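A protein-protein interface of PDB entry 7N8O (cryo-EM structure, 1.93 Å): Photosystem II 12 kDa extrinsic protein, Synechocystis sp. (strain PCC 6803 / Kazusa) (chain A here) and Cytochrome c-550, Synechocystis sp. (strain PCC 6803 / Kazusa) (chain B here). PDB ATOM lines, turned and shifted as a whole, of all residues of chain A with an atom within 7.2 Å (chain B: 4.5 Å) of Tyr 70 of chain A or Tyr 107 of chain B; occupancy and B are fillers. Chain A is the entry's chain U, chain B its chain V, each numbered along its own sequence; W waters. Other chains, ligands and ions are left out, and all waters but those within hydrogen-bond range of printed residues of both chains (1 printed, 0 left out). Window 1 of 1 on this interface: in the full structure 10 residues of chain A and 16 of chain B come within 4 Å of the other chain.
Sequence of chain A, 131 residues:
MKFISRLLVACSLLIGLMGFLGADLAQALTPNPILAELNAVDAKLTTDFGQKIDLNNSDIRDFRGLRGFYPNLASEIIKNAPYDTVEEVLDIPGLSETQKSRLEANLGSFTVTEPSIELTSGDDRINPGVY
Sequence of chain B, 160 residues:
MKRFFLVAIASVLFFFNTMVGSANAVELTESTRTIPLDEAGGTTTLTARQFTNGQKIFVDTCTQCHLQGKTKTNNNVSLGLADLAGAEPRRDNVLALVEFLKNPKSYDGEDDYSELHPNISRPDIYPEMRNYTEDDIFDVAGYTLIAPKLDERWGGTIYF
The backbone carbonyl oxygen of Asn 76 of chain B lies within hydrogen-bond range of the guanidinium group of Arg 64 of chain A, at 2.9 Å. The backbone NH (N) of Asn 72 of chain A lies within hydrogen-bond range of the side-chain carboxylate (OD2) of Asp 108 of chain B, 3.0 Å away. The side-chain hydroxyl (OH) of Tyr 70 of chain A sits at hydrogen-bond distance from the side-chain amide nitrogen (ND2) of Asn 76 of chain B (2.9 Å). N of Asp 108 of chain B lies within hydrogen-bond range of O of Tyr 70 of chain A. The guanidinium group (NH2) of Arg 64 of chain A is in salt-bridge range of the side-chain carboxylate (OD1) of Asp 83 of chain B. The guanidinium group (NH1) of Arg 67 of chain A lies within hydrogen-bond range of the backbone carbonyl oxygen (O) of Ala 87 of chain B. The backbone nitrogen of Pro 71 of chain A lies close to the side-chain carboxylate of Asp 108 of chain B (3.4 Å). The side-chain amide oxygen (OD1) of Asn 76 of chain B sits at hydrogen-bond distance from the guanidinium group (NH2) of Arg 61 of chain A (2.7 Å).
NE of Arg 64 of chain A is in hydrogen-bond range of O of Arg 61 of chain A (2.8 Å). O of Asp 83 of chain B lies within hydrogen-bond range of OH of Tyr 107 of chain B (2.5 Å). The side-chain hydroxyl (OG) of Ser 75 of chain A sits at hydrogen-bond distance from the backbone carbonyl oxygen (O) of Asn 72 of chain A, 2.7 Å away. O of Gly 68 of chain A is in hydrogen-bond range of NH1 of Arg 102 of chain A, at 2.7 Å. O of Pro 71 of chain A sits close to OG of Ser 75 of chain A (3.4 Å). OG of Ser 106 of chain B sits at hydrogen-bond distance from OD1 of Asp 108 of chain B (2.5 Å).
Among the printed residues, pairs that only touch across the chains: Arg 64 of chain A with Tyr 107 of chain B (3.7 Å), Arg 67 of chain A with Gly 86 of chain B (3.6 Å), Arg 67 of chain A with Glu 88 of chain B (3.3 Å), Gly 68 of chain A with Asp 108 of chain B (3.3 Å), Phe 69 of chain A with Asp 108 of chain B (3.7 Å), Tyr 70 of chain A with Asn 74 of chain B (3.9 Å), Tyr 70 of chain A with Val 77 of chain B (3.8 Å) and Tyr 70 of chain A with Tyr 107 of chain B (3.4 Å).
Of chain B, only Asn 74, Asn 76, Val 77, Tyr 107 and Asp 108 come within 4 Å of Tyr 70 of chain A. Of chain A, only Arg 64 (3.7 Å) and Tyr 70 (3.4 Å) come within 4 Å of Tyr 107 of chain B. Of the printed residues of chain A, Asn 74 of chain B touches Tyr 70. Printed residues of chain B within 4 Å of Arg 61 of chain A: Asn 76 (2.7 Å). Gly 109 of chain B touches none of the printed residues of chain A. Ile 126 of chain A touches none of the printed residues of chain B.
Of the 18 printed residues of chain A, 8 touch a printed residue of chain B. Hydrophobic or aromatic side chains of chain A within 4 Å of the printed part of chain B: Tyr 70 and Pro 71. Among the printed residues, 16 pairs touch across the chains. Among the printed residues, Asp or Glu carboxylates within 4 Å of a Lys or Arg side-chain nitrogen of the other chain: Arg 64 of chain A with Asp 83 of chain B.
Water W1 bridges O of Ile 126 of chain A (2.8 Å) and ND2 of Asn 76 of chain B (3.1 Å).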
ATOM      1  N   ILE A  60     -24.580  16.422 -31.126  1.00  0.00           N
ATOM      2  CA  ILE A  60     -24.386  16.756 -29.722  1.00  0.00           C
ATOM      3  C   ILE A  60     -25.443  16.092 -28.849  1.00  0.00           C
ATOM      4  O   ILE A  60     -25.177  15.744 -27.690  1.00  0.00           O
ATOM      5  CB  ILE A  60     -24.344  18.287 -29.564  1.00  0.00           C
ATOM      6  CG1 ILE A  60     -23.660  18.670 -28.260  1.00  0.00           C
ATOM      7  CG2 ILE A  60     -25.738  18.899 -29.681  1.00  0.00           C
ATOM      8  CD1 ILE A  60     -23.818  20.110 -27.897  1.00  0.00           C
ATOM      9  N   ARG A  61     -26.642  15.863 -29.394  1.00  0.00           N
ATOM     10  CA  ARG A  61     -27.669  15.155 -28.640  1.00  0.00           C
ATOM     11  C   ARG A  61     -27.175  13.793 -28.183  1.00  0.00           C
ATOM     12  O   ARG A  61     -27.533  13.337 -27.091  1.00  0.00           O
ATOM     13  CB  ARG A  61     -28.930  15.000 -29.493  1.00  0.00           C
ATOM     14  CG  ARG A  61     -29.821  16.231 -29.516  1.00  0.00           C
ATOM     15  CD  ARG A  61     -30.837  16.167 -30.649  1.00  0.00           C
ATOM     16  NE  ARG A  61     -31.809  15.091 -30.470  1.00  0.00           N
ATOM     17  CZ  ARG A  61     -32.898  15.186 -29.713  1.00  0.00           C
ATOM     18  NH1 ARG A  61     -33.724  14.155 -29.610  1.00  0.00           N
ATOM     19  NH2 ARG A  61     -33.162  16.314 -29.059  1.00  0.00           N
ATOM     20  N   ASP A  62     -26.325  13.151 -28.986  1.00  0.00           N
ATOM     21  CA  ASP A  62     -25.841  11.812 -28.689  1.00  0.00           C
ATOM     22  C   ASP A  62     -24.942  11.777 -27.465  1.00  0.00           C
ATOM     23  O   ASP A  62     -24.660  10.689 -26.955  1.00  0.00           O
ATOM     24  CB  ASP A  62     -25.109  11.248 -29.910  1.00  0.00           C
ATOM     25  CG  ASP A  62     -26.020  11.120 -31.132  1.00  0.00           C
ATOM     26  OD1 ASP A  62     -25.513  11.134 -32.273  1.00  0.00           O
ATOM     27  OD2 ASP A  62     -27.254  11.030 -30.962  1.00  0.00           O
ATOM     28  N   PHE A  63     -24.505  12.925 -26.969  1.00  0.00           N
ATOM     29  CA  PHE A  63     -23.726  12.969 -25.740  1.00  0.00           C
ATOM     30  C   PHE A  63     -24.592  13.105 -24.501  1.00  0.00           C
ATOM     31  O   PHE A  63     -24.061  13.088 -23.386  1.00  0.00           O
ATOM     32  CB  PHE A  63     -22.736  14.123 -25.804  1.00  0.00           C
ATOM     33  CG  PHE A  63     -21.592  13.882 -26.724  1.00  0.00           C
ATOM     34  CD1 PHE A  63     -21.536  14.512 -27.947  1.00  0.00           C
ATOM     35  CD2 PHE A  63     -20.543  13.063 -26.346  1.00  0.00           C
ATOM     36  CE1 PHE A  63     -20.478  14.301 -28.797  1.00  0.00           C
ATOM     37  CE2 PHE A  63     -19.475  12.855 -27.190  1.00  0.00           C
ATOM     38  CZ  PHE A  63     -19.443  13.475 -28.416  1.00  0.00           C
ATOM     39  N   ARG A  64     -25.907  13.239 -24.669  1.00  0.00           N
ATOM     40  CA  ARG A  64     -26.772  13.521 -23.532  1.00  0.00           C
ATOM     41  C   ARG A  64     -26.794  12.369 -22.541  1.00  0.00           C
ATOM     42  O   ARG A  64     -26.947  12.597 -21.339  1.00  0.00           O
ATOM     43  CB  ARG A  64     -28.186  13.848 -24.011  1.00  0.00           C
ATOM     44  CG  ARG A  64     -28.395  15.302 -24.349  1.00  0.00           C
ATOM     45  CD  ARG A  64     -29.640  15.538 -25.183  1.00  0.00           C
ATOM     46  NE  ARG A  64     -29.954  14.429 -26.075  1.00  0.00           N
ATOM     47  CZ  ARG A  64     -31.182  14.121 -26.474  1.00  0.00           C
ATOM     48  NH1 ARG A  64     -31.382  13.095 -27.290  1.00  0.00           N
ATOM     49  NH2 ARG A  64     -32.215  14.836 -26.050  1.00  0.00           N
ATOM     50  N   GLY A  65     -26.640  11.133 -23.021  1.00  0.00           N
ATOM     51  CA  GLY A  65     -26.657   9.989 -22.124  1.00  0.00           C
ATOM     52  C   GLY A  65     -25.457   9.938 -21.202  1.00  0.00           C
ATOM     53  O   GLY A  65     -25.510   9.310 -20.140  1.00  0.00           O
ATOM     54  N   LEU A  66     -24.364  10.595 -21.583  1.00  0.00           N
ATOM     55  CA  LEU A  66     -23.178  10.661 -20.738  1.00  0.00           C
ATOM     56  C   LEU A  66     -23.396  11.751 -19.702  1.00  0.00           C
ATOM     57  O   LEU A  66     -23.377  12.939 -20.032  1.00  0.00           O
ATOM     58  CB  LEU A  66     -21.931  10.933 -21.573  1.00  0.00           C
ATOM     59  CG  LEU A  66     -21.578   9.863 -22.601  1.00  0.00           C
ATOM     60  CD1 LEU A  66     -20.192  10.106 -23.144  1.00  0.00           C
ATOM     61  CD2 LEU A  66     -21.685   8.476 -21.999  1.00  0.00           C
ATOM     62  N   ARG A  67     -23.629  11.349 -18.456  1.00  0.00           N
ATOM     63  CA  ARG A  67     -23.943  12.318 -17.422  1.00  0.00           C
ATOM     64  C   ARG A  67     -22.797  13.303 -17.262  1.00  0.00           C
ATOM     65  O   ARG A  67     -21.639  12.909 -17.107  1.00  0.00           O
ATOM     66  CB  ARG A  67     -24.233  11.618 -16.096  1.00  0.00           C
ATOM     67  CG  ARG A  67     -24.711  12.570 -15.018  1.00  0.00           C
ATOM     68  CD  ARG A  67     -24.949  11.862 -13.699  1.00  0.00           C
ATOM     69  NE  ARG A  67     -25.568  10.551 -13.883  1.00  0.00           N
ATOM     70  CZ  ARG A  67     -26.877  10.358 -13.984  1.00  0.00           C
ATOM     71  NH1 ARG A  67     -27.703  11.394 -13.931  1.00  0.00           N
ATOM     72  NH2 ARG A  67     -27.364   9.135 -14.146  1.00  0.00           N
ATOM     73  N   GLY A  68     -23.127  14.587 -17.303  1.00  0.00           N
ATOM     74  CA  GLY A  68     -22.136  15.629 -17.197  1.00  0.00           C
ATOM     75  C   GLY A  68     -21.541  16.100 -18.505  1.00  0.00           C
ATOM     76  O   GLY A  68     -20.645  16.950 -18.482  1.00  0.00           O
ATOM     77  N   PHE A  69     -22.010  15.588 -19.641  1.00  0.00           N
ATOM     78  CA  PHE A  69     -21.463  15.949 -20.940  1.00  0.00           C
ATOM     79  C   PHE A  69     -22.259  17.055 -21.623  1.00  0.00           C
ATOM     80  O   PHE A  69     -21.685  18.064 -22.030  1.00  0.00           O
ATOM     81  CB  PHE A  69     -21.410  14.723 -21.851  1.00  0.00           C
ATOM     82  CG  PHE A  69     -20.088  14.021 -21.843  1.00  0.00           C
ATOM     83  CD1 PHE A  69     -19.369  13.859 -23.011  1.00  0.00           C
ATOM     84  CD2 PHE A  69     -19.579  13.498 -20.671  1.00  0.00           C
ATOM     85  CE1 PHE A  69     -18.163  13.213 -23.001  1.00  0.00           C
ATOM     86  CE2 PHE A  69     -18.372  12.844 -20.657  1.00  0.00           C
ATOM     87  CZ  PHE A  69     -17.661  12.701 -21.820  1.00  0.00           C
ATOM     88  N   TYR A  70     -23.562  16.884 -21.753  1.00  0.00           N
ATOM     89  CA  TYR A  70     -24.378  17.886 -22.422  1.00  0.00           C
ATOM     90  C   TYR A  70     -24.662  19.036 -21.468  1.00  0.00           C
ATOM     91  O   TYR A  70     -25.128  18.805 -20.352  1.00  0.00           O
ATOM     92  CB  TYR A  70     -25.688  17.286 -22.923  1.00  0.00           C
ATOM     93  CG  TYR A  70     -26.518  18.256 -23.746  1.00  0.00           C
ATOM     94  CD1 TYR A  70     -27.334  19.202 -23.139  1.00  0.00           C
ATOM     95  CD2 TYR A  70     -26.464  18.242 -25.126  1.00  0.00           C
ATOM     96  CE1 TYR A  70     -28.080  20.088 -23.888  1.00  0.00           C
ATOM     97  CE2 TYR A  70     -27.211  19.132 -25.885  1.00  0.00           C
ATOM     98  CZ  TYR A  70     -28.016  20.049 -25.257  1.00  0.00           C
ATOM     99  OH  TYR A  70     -28.758  20.936 -25.997  1.00  0.00           O
ATOM    100  N   PRO A  71     -24.438  20.281 -21.885  1.00  0.00           N
ATOM    101  CA  PRO A  71     -23.960  20.603 -23.230  1.00  0.00           C
ATOM    102  C   PRO A  71     -22.482  20.971 -23.326  1.00  0.00           C
ATOM    103  O   PRO A  71     -21.942  21.001 -24.422  1.00  0.00           O
ATOM    104  CB  PRO A  71     -24.816  21.807 -23.604  1.00  0.00           C
ATOM    105  CG  PRO A  71     -25.080  22.483 -22.305  1.00  0.00           C
ATOM    106  CD  PRO A  71     -24.981  21.464 -21.203  1.00  0.00           C
ATOM    107  N   ASN A  72     -21.841  21.244 -22.192  1.00  0.00           N
ATOM    108  CA  ASN A  72     -20.566  21.952 -22.221  1.00  0.00           C
ATOM    109  C   ASN A  72     -19.447  21.071 -22.767  1.00  0.00           C
ATOM    110  O   ASN A  72     -18.796  21.415 -23.758  1.00  0.00           O
ATOM    111  CB  ASN A  72     -20.237  22.466 -20.822  1.00  0.00           C
ATOM    112  CG  ASN A  72     -21.122  23.626 -20.416  1.00  0.00           C
ATOM    113  OD1 ASN A  72     -22.329  23.466 -20.241  1.00  0.00           O
ATOM    114  ND2 ASN A  72     -20.532  24.806 -20.291  1.00  0.00           N
ATOM    115  N   LEU A  73     -19.205  19.930 -22.123  1.00  0.00           N
ATOM    116  CA  LEU A  73     -18.154  19.028 -22.578  1.00  0.00           C
ATOM    117  C   LEU A  73     -18.446  18.486 -23.970  1.00  0.00           C
ATOM    118  O   LEU A  73     -17.531  18.313 -24.781  1.00  0.00           O
ATOM    119  CB  LEU A  73     -17.985  17.887 -21.581  1.00  0.00           C
ATOM    120  CG  LEU A  73     -16.711  17.050 -21.670  1.00  0.00           C
ATOM    121  CD1 LEU A  73     -15.488  17.923 -21.937  1.00  0.00           C
ATOM    122  CD2 LEU A  73     -16.542  16.219 -20.410  1.00  0.00           C
ATOM    123  N   ALA A  74     -19.714  18.191 -24.259  1.00  0.00           N
ATOM    124  CA  ALA A  74     -20.073  17.715 -25.590  1.00  0.00           C
ATOM    125  C   ALA A  74     -19.736  18.747 -26.654  1.00  0.00           C
ATOM    126  O   ALA A  74     -19.163  18.416 -27.701  1.00  0.00           O
ATOM    127  CB  ALA A  74     -21.559  17.370 -25.631  1.00  0.00           C
ATOM    128  N   SER A  75     -20.068  20.010 -26.392  1.00  0.00           N
ATOM    129  CA  SER A  75     -19.724  21.072 -27.323  1.00  0.00           C
ATOM    130  C   SER A  75     -18.217  21.190 -27.476  1.00  0.00           C
ATOM    131  O   SER A  75     -17.717  21.380 -28.585  1.00  0.00           O
ATOM    132  CB  SER A  75     -20.321  22.396 -26.854  1.00  0.00           C
ATOM    133  OG  SER A  75     -19.558  22.955 -25.804  1.00  0.00           O
ATOM    134  N   ARG A 102     -14.223  13.187 -16.296  1.00  0.00           N
ATOM    135  CA  ARG A 102     -15.413  12.668 -16.962  1.00  0.00           C
ATOM    136  C   ARG A 102     -15.046  11.978 -18.268  1.00  0.00           C
ATOM    137  O   ARG A 102     -15.591  10.917 -18.599  1.00  0.00           O
ATOM    138  CB  ARG A 102     -16.406  13.801 -17.215  1.00  0.00           C
ATOM    139  CG  ARG A 102     -17.192  14.197 -15.985  1.00  0.00           C
ATOM    140  CD  ARG A 102     -18.658  14.345 -16.313  1.00  0.00           C
ATOM    141  NE  ARG A 102     -19.000  15.704 -16.715  1.00  0.00           N
ATOM    142  CZ  ARG A 102     -18.973  16.758 -15.908  1.00  0.00           C
ATOM    143  NH1 ARG A 102     -19.306  17.955 -16.369  1.00  0.00           N
ATOM    144  NH2 ARG A 102     -18.641  16.618 -14.633  1.00  0.00           N
ATOM    145  N   ILE A 126     -24.475  19.971 -34.464  1.00  0.00           N
ATOM    146  CA  ILE A 126     -25.112  20.790 -33.435  1.00  0.00           C
ATOM    147  C   ILE A 126     -26.628  20.785 -33.584  1.00  0.00           C
ATOM    148  O   ILE A 126     -27.358  20.743 -32.592  1.00  0.00           O
ATOM    149  CB  ILE A 126     -24.554  22.228 -33.488  1.00  0.00           C
ATOM    150  CG1 ILE A 126     -23.113  22.273 -32.974  1.00  0.00           C
ATOM    151  CG2 ILE A 126     -25.470  23.197 -32.719  1.00  0.00           C
ATOM    152  CD1 ILE A 126     -22.931  21.732 -31.577  1.00  0.00           C
ATOM    153  N   ASN B  74     -36.066  24.236 -25.962  1.00  0.00           N
ATOM    154  CA  ASN B  74     -34.893  23.385 -26.151  1.00  0.00           C
ATOM    155  C   ASN B  74     -35.318  21.950 -25.847  1.00  0.00           C
ATOM    156  O   ASN B  74     -35.276  21.533 -24.689  1.00  0.00           O
ATOM    157  CB  ASN B  74     -33.756  23.839 -25.252  1.00  0.00           C
ATOM    158  CG  ASN B  74     -32.512  23.007 -25.411  1.00  0.00           C
ATOM    159  OD1 ASN B  74     -32.389  22.215 -26.335  1.00  0.00           O
ATOM    160  ND2 ASN B  74     -31.573  23.187 -24.498  1.00  0.00           N
ATOM    161  N   ASN B  76     -33.779  19.236 -26.587  1.00  0.00           N
ATOM    162  CA  ASN B  76     -32.706  18.350 -26.155  1.00  0.00           C
ATOM    163  C   ASN B  76     -32.784  18.060 -24.665  1.00  0.00           C
ATOM    164  O   ASN B  76     -32.238  17.052 -24.213  1.00  0.00           O
ATOM    165  CB  ASN B  76     -31.341  18.952 -26.478  1.00  0.00           C
ATOM    166  CG  ASN B  76     -31.103  19.102 -27.956  1.00  0.00           C
ATOM    167  OD1 ASN B  76     -31.907  18.665 -28.773  1.00  0.00           O
ATOM    168  ND2 ASN B  76     -29.992  19.727 -28.311  1.00  0.00           N
ATOM    169  N   VAL B  77     -33.439  18.924 -23.899  1.00  0.00           N
ATOM    170  CA  VAL B  77     -33.583  18.763 -22.454  1.00  0.00           C
ATOM    171  C   VAL B  77     -35.084  18.764 -22.175  1.00  0.00           C
ATOM    172  O   VAL B  77     -35.677  19.807 -21.898  1.00  0.00           O
ATOM    173  CB  VAL B  77     -32.875  19.871 -21.667  1.00  0.00           C
ATOM    174  CG1 VAL B  77     -32.798  19.523 -20.198  1.00  0.00           C
ATOM    175  CG2 VAL B  77     -31.485  20.141 -22.226  1.00  0.00           C
ATOM    176  N   ALA B  82     -36.013   9.579 -18.968  1.00  0.00           N
ATOM    177  CA  ALA B  82     -34.625   9.382 -19.374  1.00  0.00           C
ATOM    178  C   ALA B  82     -33.846  10.689 -19.324  1.00  0.00           C
ATOM    179  O   ALA B  82     -32.717  10.728 -18.816  1.00  0.00           O
ATOM    180  CB  ALA B  82     -34.570   8.774 -20.774  1.00  0.00           C
ATOM    181  N   ASP B  83     -34.437  11.776 -19.823  1.00  0.00           N
ATOM    182  CA  ASP B  83     -33.774  13.074 -19.751  1.00  0.00           C
ATOM    183  C   ASP B  83     -33.603  13.520 -18.306  1.00  0.00           C
ATOM    184  O   ASP B  83     -32.529  13.981 -17.915  1.00  0.00           O
ATOM    185  CB  ASP B  83     -34.546  14.114 -20.561  1.00  0.00           C
ATOM    186  CG  ASP B  83     -34.387  13.923 -22.058  1.00  0.00           C
ATOM    187  OD1 ASP B  83     -34.455  14.929 -22.797  1.00  0.00           O
ATOM    188  OD2 ASP B  83     -34.193  12.771 -22.497  1.00  0.00           O
ATOM    189  N   GLY B  86     -30.862  11.638 -16.716  1.00  0.00           N
ATOM    190  CA  GLY B  86     -29.558  11.856 -17.308  1.00  0.00           C
ATOM    191  C   GLY B  86     -28.860  13.135 -16.911  1.00  0.00           C
ATOM    192  O   GLY B  86     -27.681  13.296 -17.234  1.00  0.00           O
ATOM    193  N   ALA B  87     -29.552  14.047 -16.237  1.00  0.00           N
ATOM    194  CA  ALA B  87     -28.937  15.290 -15.804  1.00  0.00           C
ATOM    195  C   ALA B  87     -27.921  15.030 -14.702  1.00  0.00           C
ATOM    196  O   ALA B  87     -27.877  13.959 -14.096  1.00  0.00           O
ATOM    197  CB  ALA B  87     -29.986  16.277 -15.303  1.00  0.00           C
ATOM    198  N   GLU B  88     -27.098  16.036 -14.447  1.00  0.00           N
ATOM    199  CA  GLU B  88     -26.094  15.981 -13.389  1.00  0.00           C
ATOM    200  C   GLU B  88     -26.397  17.047 -12.350  1.00  0.00           C
ATOM    201  O   GLU B  88     -26.258  18.250 -12.643  1.00  0.00           O
ATOM    202  CB  GLU B  88     -24.688  16.168 -13.958  1.00  0.00           C
ATOM    203  CG  GLU B  88     -23.659  16.639 -12.938  1.00  0.00           C
ATOM    204  CD  GLU B  88     -23.230  15.547 -11.980  1.00  0.00           C
ATOM    205  OE1 GLU B  88     -22.331  15.803 -11.151  1.00  0.00           O
ATOM    206  OE2 GLU B  88     -23.783  14.431 -12.053  1.00  0.00           O
ATOM    207  N   ARG B  91     -32.159  14.261 -11.837  1.00  0.00           N
ATOM    208  CA  ARG B  91     -33.347  15.019 -11.485  1.00  0.00           C
ATOM    209  C   ARG B  91     -34.604  14.161 -11.514  1.00  0.00           C
ATOM    210  O   ARG B  91     -35.709  14.701 -11.573  1.00  0.00           O
ATOM    211  CB  ARG B  91     -33.504  16.219 -12.417  1.00  0.00           C
ATOM    212  CG  ARG B  91     -32.231  17.023 -12.586  1.00  0.00           C
ATOM    213  CD  ARG B  91     -32.467  18.280 -13.388  1.00  0.00           C
ATOM    214  NE  ARG B  91     -31.321  19.180 -13.338  1.00  0.00           N
ATOM    215  CZ  ARG B  91     -30.878  19.881 -14.374  1.00  0.00           C
ATOM    216  NH1 ARG B  91     -31.481  19.792 -15.551  1.00  0.00           N
ATOM    217  NH2 ARG B  91     -29.833  20.675 -14.235  1.00  0.00           N
ATOM    218  N   LYS B 105     -29.956  24.997 -13.333  1.00  0.00           N
ATOM    219  CA  LYS B 105     -28.605  24.847 -13.854  1.00  0.00           C
ATOM    220  C   LYS B 105     -28.677  24.209 -15.232  1.00  0.00           C
ATOM    221  O   LYS B 105     -29.721  23.716 -15.659  1.00  0.00           O
ATOM    222  CB  LYS B 105     -27.737  23.983 -12.934  1.00  0.00           C
ATOM    223  CG  LYS B 105     -27.681  24.442 -11.492  1.00  0.00           C
ATOM    224  CD  LYS B 105     -27.362  25.918 -11.375  1.00  0.00           C
ATOM    225  CE  LYS B 105     -25.872  26.171 -11.421  1.00  0.00           C
ATOM    226  NZ  LYS B 105     -25.261  25.950 -10.084  1.00  0.00           N
ATOM    227  N   SER B 106     -27.549  24.218 -15.929  1.00  0.00           N
ATOM    228  CA  SER B 106     -27.466  23.496 -17.183  1.00  0.00           C
ATOM    229  C   SER B 106     -27.564  21.994 -16.927  1.00  0.00           C
ATOM    230  O   SER B 106     -27.462  21.523 -15.796  1.00  0.00           O
ATOM    231  CB  SER B 106     -26.167  23.826 -17.911  1.00  0.00           C
ATOM    232  OG  SER B 106     -25.066  23.199 -17.279  1.00  0.00           O
ATOM    233  N   TYR B 107     -27.763  21.246 -18.011  1.00  0.00           N
ATOM    234  CA  TYR B 107     -28.032  19.815 -17.906  1.00  0.00           C
ATOM    235  C   TYR B 107     -26.870  19.057 -17.283  1.00  0.00           C
ATOM    236  O   TYR B 107     -27.089  18.109 -16.527  1.00  0.00           O
ATOM    237  CB  TYR B 107     -28.345  19.253 -19.284  1.00  0.00           C
ATOM    238  CG  TYR B 107     -28.917  17.863 -19.285  1.00  0.00           C
ATOM    239  CD1 TYR B 107     -30.159  17.605 -18.726  1.00  0.00           C
ATOM    240  CD2 TYR B 107     -28.226  16.810 -19.867  1.00  0.00           C
ATOM    241  CE1 TYR B 107     -30.691  16.342 -18.734  1.00  0.00           C
ATOM    242  CE2 TYR B 107     -28.759  15.541 -19.889  1.00  0.00           C
ATOM    243  CZ  TYR B 107     -29.990  15.311 -19.319  1.00  0.00           C
ATOM    244  OH  TYR B 107     -30.519  14.047 -19.332  1.00  0.00           O
ATOM    245  N   ASP B 108     -25.638  19.430 -17.616  1.00  0.00           N
ATOM    246  CA  ASP B 108     -24.462  18.878 -16.960  1.00  0.00           C
ATOM    247  C   ASP B 108     -24.177  19.555 -15.630  1.00  0.00           C
ATOM    248  O   ASP B 108     -23.129  19.301 -15.031  1.00  0.00           O
ATOM    249  CB  ASP B 108     -23.243  18.974 -17.880  1.00  0.00           C
ATOM    250  CG  ASP B 108     -22.953  20.390 -18.331  1.00  0.00           C
ATOM    251  OD1 ASP B 108     -23.480  21.341 -17.732  1.00  0.00           O
ATOM    252  OD2 ASP B 108     -22.179  20.551 -19.295  1.00  0.00           O
ATOM    253  N   GLY B 109     -25.087  20.407 -15.165  1.00  0.00           N
ATOM    254  CA  GLY B 109     -24.896  21.106 -13.908  1.00  0.00           C
ATOM    255  C   GLY B 109     -23.664  21.975 -13.869  1.00  0.00           C
ATOM    256  O   GLY B 109     -23.009  22.058 -12.826  1.00  0.00           O
HETATM  257  O   HOH W   1     -29.546  19.551 -31.365  1.00  0.00           O
